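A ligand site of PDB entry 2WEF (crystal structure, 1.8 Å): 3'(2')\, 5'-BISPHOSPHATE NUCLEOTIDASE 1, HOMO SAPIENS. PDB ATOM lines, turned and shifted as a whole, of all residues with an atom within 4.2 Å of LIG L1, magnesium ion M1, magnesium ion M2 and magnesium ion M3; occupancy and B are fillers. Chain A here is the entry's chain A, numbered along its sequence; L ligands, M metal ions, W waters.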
ATOM      1  N   LYS A  36      -0.245  35.115  15.811  1.00  0.00           N
ATOM      2  CA  LYS A  36       0.415  35.532  14.567  1.00  0.00           C
ATOM      3  C   LYS A  36      -0.709  35.976  13.622  1.00  0.00           C
ATOM      4  O   LYS A  36      -1.204  37.091  13.791  1.00  0.00           O
ATOM      5  CB  LYS A  36       1.327  34.473  14.022  1.00  0.00           C
ATOM      6  CG  LYS A  36       2.571  34.369  14.971  1.00  0.00           C
ATOM      7  CD  LYS A  36       3.731  33.510  14.474  1.00  0.00           C
ATOM      8  CE  LYS A  36       3.337  32.115  14.116  1.00  0.00           C
ATOM      9  NZ  LYS A  36       4.434  31.490  13.350  1.00  0.00           N
ATOM     10  N   ASP A  41      -3.282  30.479  15.176  1.00  0.00           N
ATOM     11  CA  ASP A  41      -1.911  30.543  14.591  1.00  0.00           C
ATOM     12  C   ASP A  41      -1.051  31.199  15.682  1.00  0.00           C
ATOM     13  O   ASP A  41      -0.860  32.448  15.694  1.00  0.00           O
ATOM     14  CB  ASP A  41      -1.942  31.351  13.263  1.00  0.00           C
ATOM     15  CG  ASP A  41      -0.568  31.535  12.575  1.00  0.00           C
ATOM     16  OD1 ASP A  41       0.344  30.685  12.795  1.00  0.00           O
ATOM     17  OD2 ASP A  41      -0.382  32.567  11.834  1.00  0.00           O
ATOM     18  N   ASP A  47       8.114  27.872  21.578  1.00  0.00           N
ATOM     19  CA  ASP A  47       8.444  27.952  20.150  1.00  0.00           C
ATOM     20  C   ASP A  47       9.688  28.753  19.950  1.00  0.00           C
ATOM     21  O   ASP A  47      10.607  28.364  19.238  1.00  0.00           O
ATOM     22  CB  ASP A  47       7.355  28.506  19.287  1.00  0.00           C
ATOM     23  CG  ASP A  47       6.008  27.740  19.414  1.00  0.00           C
ATOM     24  OD1 ASP A  47       5.298  27.980  20.408  1.00  0.00           O
ATOM     25  OD2 ASP A  47       5.644  26.924  18.542  1.00  0.00           O
ATOM     26  N   GLU A  70      10.528  27.545  11.299  1.00  0.00           N
ATOM     27  CA  GLU A  70       9.206  28.137  11.142  1.00  0.00           C
ATOM     28  C   GLU A  70       9.065  29.602  11.565  1.00  0.00           C
ATOM     29  O   GLU A  70       8.467  30.440  10.832  1.00  0.00           O
ATOM     30  CB  GLU A  70       8.210  27.353  11.964  1.00  0.00           C
ATOM     31  CG  GLU A  70       6.813  27.875  11.866  1.00  0.00           C
ATOM     32  CD  GLU A  70       5.798  27.161  12.686  1.00  0.00           C
ATOM     33  OE1 GLU A  70       6.134  26.219  13.400  1.00  0.00           O
ATOM     34  OE2 GLU A  70       4.618  27.505  12.527  1.00  0.00           O
ATOM     35  N   GLU A  71       9.597  29.911  12.737  1.00  0.00           N
ATOM     36  CA  GLU A  71       9.353  31.179  13.391  1.00  0.00           C
ATOM     37  C   GLU A  71      10.276  32.258  12.801  1.00  0.00           C
ATOM     38  O   GLU A  71      11.442  32.019  12.498  1.00  0.00           O
ATOM     39  CB  GLU A  71       9.514  31.062  14.888  1.00  0.00           C
ATOM     40  CG  GLU A  71       8.620  29.961  15.518  1.00  0.00           C
ATOM     41  CD  GLU A  71       7.111  30.041  15.254  1.00  0.00           C
ATOM     42  OE1 GLU A  71       6.515  31.177  15.106  1.00  0.00           O
ATOM     43  OE2 GLU A  71       6.479  28.955  15.244  1.00  0.00           O
ATOM     44  N   ASP A 113      10.778  22.638  12.665  1.00  0.00           N
ATOM     45  CA  ASP A 113       9.609  23.038  13.354  1.00  0.00           C
ATOM     46  C   ASP A 113       9.897  22.859  14.796  1.00  0.00           C
ATOM     47  O   ASP A 113       9.940  21.747  15.279  1.00  0.00           O
ATOM     48  CB  ASP A 113       8.379  22.233  12.923  1.00  0.00           C
ATOM     49  CG  ASP A 113       7.086  22.881  13.413  1.00  0.00           C
ATOM     50  OD1 ASP A 113       7.112  23.654  14.373  1.00  0.00           O
ATOM     51  OD2 ASP A 113       6.073  22.550  12.809  1.00  0.00           O
ATOM     52  N   LEU A 115       8.388  23.551  17.456  1.00  0.00           N
ATOM     53  CA  LEU A 115       7.265  23.045  18.270  1.00  0.00           C
ATOM     54  C   LEU A 115       6.117  22.950  17.293  1.00  0.00           C
ATOM     55  O   LEU A 115       5.636  23.971  16.802  1.00  0.00           O
ATOM     56  CB  LEU A 115       6.942  23.995  19.454  1.00  0.00           C
ATOM     57  CG  LEU A 115       6.126  23.422  20.560  1.00  0.00           C
ATOM     58  CD1 LEU A 115       6.032  24.445  21.749  1.00  0.00           C
ATOM     59  CD2 LEU A 115       4.710  23.017  20.055  1.00  0.00           C
ATOM     60  N   ASP A 116       5.689  21.734  17.015  1.00  0.00           N
ATOM     61  CA  ASP A 116       4.570  21.429  16.141  1.00  0.00           C
ATOM     62  C   ASP A 116       3.423  21.000  16.965  1.00  0.00           C
ATOM     63  O   ASP A 116       3.545  20.083  17.796  1.00  0.00           O
ATOM     64  CB  ASP A 116       4.914  20.361  15.061  1.00  0.00           C
ATOM     65  CG  ASP A 116       3.768  20.131  14.104  1.00  0.00           C
ATOM     66  OD1 ASP A 116       3.412  21.126  13.422  1.00  0.00           O
ATOM     67  OD2 ASP A 116       3.284  18.949  14.030  1.00  0.00           O
ATOM     68  N   THR A 118       1.432  23.751  18.370  1.00  0.00           N
ATOM     69  CA  THR A 118       1.415  24.841  19.344  1.00  0.00           C
ATOM     70  C   THR A 118      -0.008  25.187  19.907  1.00  0.00           C
ATOM     71  O   THR A 118      -0.193  25.445  21.130  1.00  0.00           O
ATOM     72  CB  THR A 118       2.061  26.078  18.727  1.00  0.00           C
ATOM     73  OG1 THR A 118       3.364  25.820  18.250  1.00  0.00           O
ATOM     74  CG2 THR A 118       2.056  27.252  19.729  1.00  0.00           C
ATOM     75  N   THR A 191      -6.805  17.469  11.056  1.00  0.00           N
ATOM     76  CA  THR A 191      -6.674  18.636  11.919  1.00  0.00           C
ATOM     77  C   THR A 191      -7.815  18.748  12.944  1.00  0.00           C
ATOM     78  O   THR A 191      -8.947  18.356  12.672  1.00  0.00           O
ATOM     79  CB  THR A 191      -6.649  19.917  11.031  1.00  0.00           C
ATOM     80  OG1 THR A 191      -6.535  21.100  11.854  1.00  0.00           O
ATOM     81  CG2 THR A 191      -7.932  19.974  10.143  1.00  0.00           C
ATOM     82  N   HIS A 194      -7.668  23.562  12.488  1.00  0.00           N
ATOM     83  CA  HIS A 194      -7.575  24.251  11.234  1.00  0.00           C
ATOM     84  C   HIS A 194      -8.481  23.598  10.184  1.00  0.00           C
ATOM     85  O   HIS A 194      -8.129  23.520   9.030  1.00  0.00           O
ATOM     86  CB  HIS A 194      -6.104  24.335  10.744  1.00  0.00           C
ATOM     87  CG  HIS A 194      -5.188  24.948  11.768  1.00  0.00           C
ATOM     88  ND1 HIS A 194      -4.253  24.225  12.493  1.00  0.00           N
ATOM     89  CD2 HIS A 194      -5.108  26.223  12.221  1.00  0.00           C
ATOM     90  CE1 HIS A 194      -3.668  25.037  13.366  1.00  0.00           C
ATOM     91  NE2 HIS A 194      -4.157  26.258  13.206  1.00  0.00           N
ATOM     92  N   VAL A 214      -6.898  15.576  15.945  1.00  0.00           N
ATOM     93  CA  VAL A 214      -5.747  15.807  16.786  1.00  0.00           C
ATOM     94  C   VAL A 214      -4.897  16.885  16.144  1.00  0.00           C
ATOM     95  O   VAL A 214      -4.922  17.114  14.908  1.00  0.00           O
ATOM     96  CB  VAL A 214      -4.904  14.528  17.009  1.00  0.00           C
ATOM     97  CG1 VAL A 214      -5.797  13.396  17.688  1.00  0.00           C
ATOM     98  CG2 VAL A 214      -4.290  14.026  15.686  1.00  0.00           C
ATOM     99  N   GLY A 215      -4.118  17.567  16.981  1.00  0.00           N
ATOM    100  CA  GLY A 215      -3.202  18.520  16.470  1.00  0.00           C
ATOM    101  C   GLY A 215      -1.845  17.899  16.058  1.00  0.00           C
ATOM    102  O   GLY A 215      -1.475  16.895  16.532  1.00  0.00           O
ATOM    103  N   GLY A 216      -1.148  18.601  15.184  1.00  0.00           N
ATOM    104  CA  GLY A 216       0.225  18.319  14.804  1.00  0.00           C
ATOM    105  C   GLY A 216       0.392  17.406  13.611  1.00  0.00           C
ATOM    106  O   GLY A 216      -0.257  16.340  13.491  1.00  0.00           O
ATOM    107  N   ALA A 217       1.224  17.849  12.670  1.00  0.00           N
ATOM    108  CA  ALA A 217       1.673  17.016  11.540  1.00  0.00           C
ATOM    109  C   ALA A 217       2.577  15.845  12.024  1.00  0.00           C
ATOM    110  O   ALA A 217       2.426  14.710  11.556  1.00  0.00           O
ATOM    111  CB  ALA A 217       2.405  17.886  10.492  1.00  0.00           C
ATOM    112  N   LYS A 220       0.418  13.209  13.729  1.00  0.00           N
ATOM    113  CA  LYS A 220      -0.427  12.386  12.831  1.00  0.00           C
ATOM    114  C   LYS A 220       0.387  11.349  12.078  1.00  0.00           C
ATOM    115  O   LYS A 220      -0.114  10.298  11.822  1.00  0.00           O
ATOM    116  CB  LYS A 220      -1.311  13.263  11.936  1.00  0.00           C
ATOM    117  CG  LYS A 220      -2.494  13.862  12.735  1.00  0.00           C
ATOM    118  CD  LYS A 220      -3.544  14.690  11.947  1.00  0.00           C
ATOM    119  CE  LYS A 220      -3.152  16.068  11.615  1.00  0.00           C
ATOM    120  NZ  LYS A 220      -3.065  16.881  12.914  1.00  0.00           N
ATOM    121  N   PHE A 234      -5.481  15.892   4.791  1.00  0.00           N
ATOM    122  CA  PHE A 234      -5.591  17.331   5.079  1.00  0.00           C
ATOM    123  C   PHE A 234      -5.662  18.123   3.744  1.00  0.00           C
ATOM    124  O   PHE A 234      -4.658  18.523   3.183  1.00  0.00           O
ATOM    125  CB  PHE A 234      -4.375  17.764   5.898  1.00  0.00           C
ATOM    126  CG  PHE A 234      -4.424  19.191   6.307  1.00  0.00           C
ATOM    127  CD1 PHE A 234      -5.526  19.656   7.030  1.00  0.00           C
ATOM    128  CD2 PHE A 234      -3.378  20.029   6.039  1.00  0.00           C
ATOM    129  CE1 PHE A 234      -5.561  21.032   7.471  1.00  0.00           C
ATOM    130  CE2 PHE A 234      -3.390  21.360   6.420  1.00  0.00           C
ATOM    131  CZ  PHE A 234      -4.498  21.875   7.139  1.00  0.00           C
ATOM    132  N   GLY A 238      -1.762  25.352   4.511  1.00  0.00           N
ATOM    133  CA  GLY A 238      -1.629  25.599   5.943  1.00  0.00           C
ATOM    134  C   GLY A 238      -0.409  25.004   6.533  1.00  0.00           C
ATOM    135  O   GLY A 238       0.247  25.601   7.376  1.00  0.00           O
ATOM    136  N   CYS A 239      -0.092  23.804   6.098  1.00  0.00           N
ATOM    137  CA  CYS A 239       1.091  23.234   6.602  1.00  0.00           C
ATOM    138  C   CYS A 239       2.254  23.530   5.642  1.00  0.00           C
ATOM    139  O   CYS A 239       2.020  23.906   4.512  1.00  0.00           O
ATOM    140  CB  CYS A 239       0.912  21.834   6.973  1.00  0.00           C
ATOM    141  SG  CYS A 239       1.066  20.683   5.714  1.00  0.00           S
ATOM    142  N   ASP A 243       6.756  21.049   8.564  1.00  0.00           N
ATOM    143  CA  ASP A 243       5.743  20.152   9.135  1.00  0.00           C
ATOM    144  C   ASP A 243       5.865  18.768   8.538  1.00  0.00           C
ATOM    145  O   ASP A 243       5.540  17.750   9.186  1.00  0.00           O
ATOM    146  CB  ASP A 243       4.313  20.715   8.803  1.00  0.00           C
ATOM    147  CG  ASP A 243       4.004  21.959   9.570  1.00  0.00           C
ATOM    148  OD1 ASP A 243       4.005  21.837  10.784  1.00  0.00           O
ATOM    149  OD2 ASP A 243       3.791  23.042   8.964  1.00  0.00           O
HETATM  150  P1  LIG L   1      -2.873  20.675  12.356  1.00  0.00           P
HETATM  151  O1  LIG L   1      -3.276  19.320  11.816  1.00  0.00           O
HETATM  152  O2  LIG L   1      -4.000  21.627  12.263  1.00  0.00           O
HETATM  153  O3  LIG L   1      -2.153  20.709  13.657  1.00  0.00           O
HETATM  154  O4  LIG L   1      -1.879  21.269  11.263  1.00  0.00           O
HETATM  155  C1  LIG L   1      -0.575  20.706  11.028  1.00  0.00           C
HETATM  156  C2  LIG L   1       0.498  21.784  11.040  1.00  0.00           C
HETATM  157  O5  LIG L   1       0.257  22.754  10.045  1.00  0.00           O
HETATM  158  C3  LIG L   1       0.557  22.667  12.326  1.00  0.00           C
HETATM  159  O6  LIG L   1       1.809  23.439  12.378  1.00  0.00           O
HETATM  160  C4  LIG L   1      -0.387  23.765  12.092  1.00  0.00           C
HETATM  161  O7  LIG L   1      -0.143  24.873  12.952  1.00  0.00           O
HETATM  162  C5  LIG L   1      -0.048  24.017  10.628  1.00  0.00           C
HETATM  163  N1  LIG L   1      -1.265  24.540  10.052  1.00  0.00           N
HETATM  164  C6  LIG L   1      -2.221  23.846   9.415  1.00  0.00           C
HETATM  165  N2  LIG L   1      -3.183  24.656   8.979  1.00  0.00           N
HETATM  166  C7  LIG L   1      -2.856  25.901   9.414  1.00  0.00           C
HETATM  167  C8  LIG L   1      -3.449  27.240   9.329  1.00  0.00           C
HETATM  168  N3  LIG L   1      -4.622  27.434   8.722  1.00  0.00           N
HETATM  169  N4  LIG L   1      -2.761  28.266   9.904  1.00  0.00           N
HETATM  170  C9  LIG L   1      -1.585  28.093  10.518  1.00  0.00           C
HETATM  171  N5  LIG L   1      -0.979  26.902  10.623  1.00  0.00           N
HETATM  172  C10 LIG L   1      -1.578  25.815  10.080  1.00  0.00           C
HETATM  173  P1  LG2 L   2       2.981  24.991  14.751  1.00  0.00           P
HETATM  174  O1  LG2 L   2       2.309  25.901  13.709  1.00  0.00           O
HETATM  175  O2  LG2 L   2       1.919  24.219  15.549  1.00  0.00           O
HETATM  176  O3  LG2 L   2       4.058  24.074  14.094  1.00  0.00           O
HETATM  177  O4  LG2 L   2       3.819  25.966  15.693  1.00  0.00           O
HETATM  178 MG    MG M   1       4.033  22.868  12.535  1.00  0.00          MG
HETATM  179 MG    MG M   2       5.699  25.018  15.009  1.00  0.00          MG
HETATM  180 MG    MG M   3       2.709  27.770  13.118  1.00  0.00          MG
HETATM  181  O   HOH W   1       2.677  29.580  12.127  1.00  0.00           O
HETATM  182  O   HOH W   2       1.160  27.761   8.505  1.00  0.00           O
HETATM  183  O   HOH W   3       6.779  26.390  16.155  1.00  0.00           O
HETATM  184  O   HOH W   4      -5.155  20.981  14.925  1.00  0.00           O
HETATM  185  O   HOH W   5      -0.654  24.792  16.051  1.00  0.00           O
HETATM  186  O   HOH W   6       2.018  26.960  11.180  1.00  0.00           O
HETATM  187  O   HOH W   7       0.768  28.306  13.539  1.00  0.00           O
HETATM  188  O   HOH W   8      -3.154  18.785   9.343  1.00  0.00           O
HETATM  189  O   HOH W   9       3.540  28.757  14.824  1.00  0.00           O
HETATM  190  O   HOH W  10       4.161  24.652  11.139  1.00  0.00           O
HETATM  191  O   HOH W  11      -6.273  24.901   7.081  1.00  0.00           O
HETATM  192  O   HOH W  12      -2.313  22.707  15.333  1.00  0.00           O
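Magnesium ion M1 is bound by O3 of LG2 L2 (2.0 Å), OD1 of Asp 243 (2.0 Å), OD1 of Asp 116 (2.1 Å), OD2 of Asp 113 (2.1 Å), water W10 (2.3 Å) and O6 of LIG L1 (2.3 Å). Magnesium ion M1 has six donor atoms within binding distance.
Of the 20 residues printed, 3 come within 4 Å of magnesium ion M1. The nearest printed residue that does not touch magnesium ion M1 is Glu 70 (4.05 Å).
The side-chain carboxylate (OE1) of Glu 70 is bound to magnesium ion M2 (2.1 Å). The side-chain carboxylate (OD1) of Asp 113 binds magnesium ion M2, at 2.1 Å. Magnesium ion M2 is bound by O of Leu 115, 2.1 Å away. Water W3 is bound to magnesium ion M2 (2.1 Å). An oxygen (O3) of LG2 L2 is bound to magnesium ion M2, 2.1 Å away. O4 of LG2 L2 binds magnesium ion M2, 2.2 Å away. Magnesium ion M2 has six donor atoms within binding distance.
An oxygen (O2) of LIG L1 sits at hydrogen-bond distance from a ring nitrogen (ND1) of His 194, 2.6 Å away. The side-chain hydroxyl of Thr 191 is in hydrogen-bond range of an oxygen (O2) of LIG L1 (2.6 Å). The side-chain amino group (NZ) of Lys 220 is in salt-bridge range of an oxygen (O1) of LIG L1. The backbone NH (N) of Gly 216 sits at hydrogen-bond distance from an oxygen (O3) of LIG L1 (2.8 Å).
Water W3 lies within hydrogen-bond range of OD2 of Asp 47 (2.7 Å) and OE2 of Glu 71 (2.7 Å). Water W9 lies within hydrogen-bond range of OE2 of Glu 71 (3.0 Å) and NZ of Lys 36 (3.2 Å). Water W4 lies within hydrogen-bond range of O2 of LIG L1 (3.0 Å) and OG1 of Thr 191 (3.4 Å). Water W2 lies within hydrogen-bond range of O of Gly 238 (2.6 Å) and N5 of LIG L1 (3.1 Å). Water W5 lies within hydrogen-bond range of an oxygen (O7) of LIG L1 (3.1 Å) and the backbone NH (N) of Thr 118 (3.3 Å). Water W11 bridges the backbone carbonyl oxygen of His 194 and a nitrogen (N3) of LIG L1.
Four residues have an atom within 4 Å of magnesium ion M2: Glu 70, Asp 113, Leu 115 and Asp 116.
OD2 of Asp 116 lies within hydrogen-bond range of N of Ala 217, at 2.7 Å. The side-chain hydroxyl (OG1) of Thr 118 sits close to the backbone carbonyl oxygen (O) of Leu 115. The backbone NH of His 194 is in hydrogen-bond range of the side-chain hydroxyl of Thr 191 (2.8 Å). The side-chain amino group (NZ) of Lys 220 sits at hydrogen-bond distance from the backbone carbonyl oxygen (O) of Gly 216 (2.9 Å). NZ of Lys 220 is in hydrogen-bond range of O of Val 214. N of Lys 36 sits at hydrogen-bond distance from O of Asp 41 (2.7 Å).
N1 of LIG L1 lies close to O of Gly 238 (3.3 Å). OD1 of Asp 41 touches C9 of LIG L1, 3.95 Å away. Gly 215 touches LIG L1. N of Ala 217 touches C1 of LIG L1 (3.8 Å). Phe 234 touches LIG L1. CB of Cys 239 touches O5 of LIG L1, at 3.3 Å. Hydrophobic or aromatic side chains within 4 Å of LIG L1: His 194 and Phe 234. 12 residues have an atom within 4 Å of LIG L1: Asp 41, Asp 116, Thr 191, His 194, Gly 215, Gly 216, Ala 217, Lys 220, Phe 234, Gly 238, Cys 239 and Asp 243.
Asp 41 touches magnesium ion M3. Within 4 Å of magnesium ion M3: Asp 41 and Glu 70.
Magnesium ion M3 is bound by O1 of LG2 L2 (2.0 Å), OE2 of Glu 70 (2.0 Å), water W7 (2.1 Å), water W1 (2.1 Å), water W9 (2.1 Å) and water W6 (2.2 Å).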
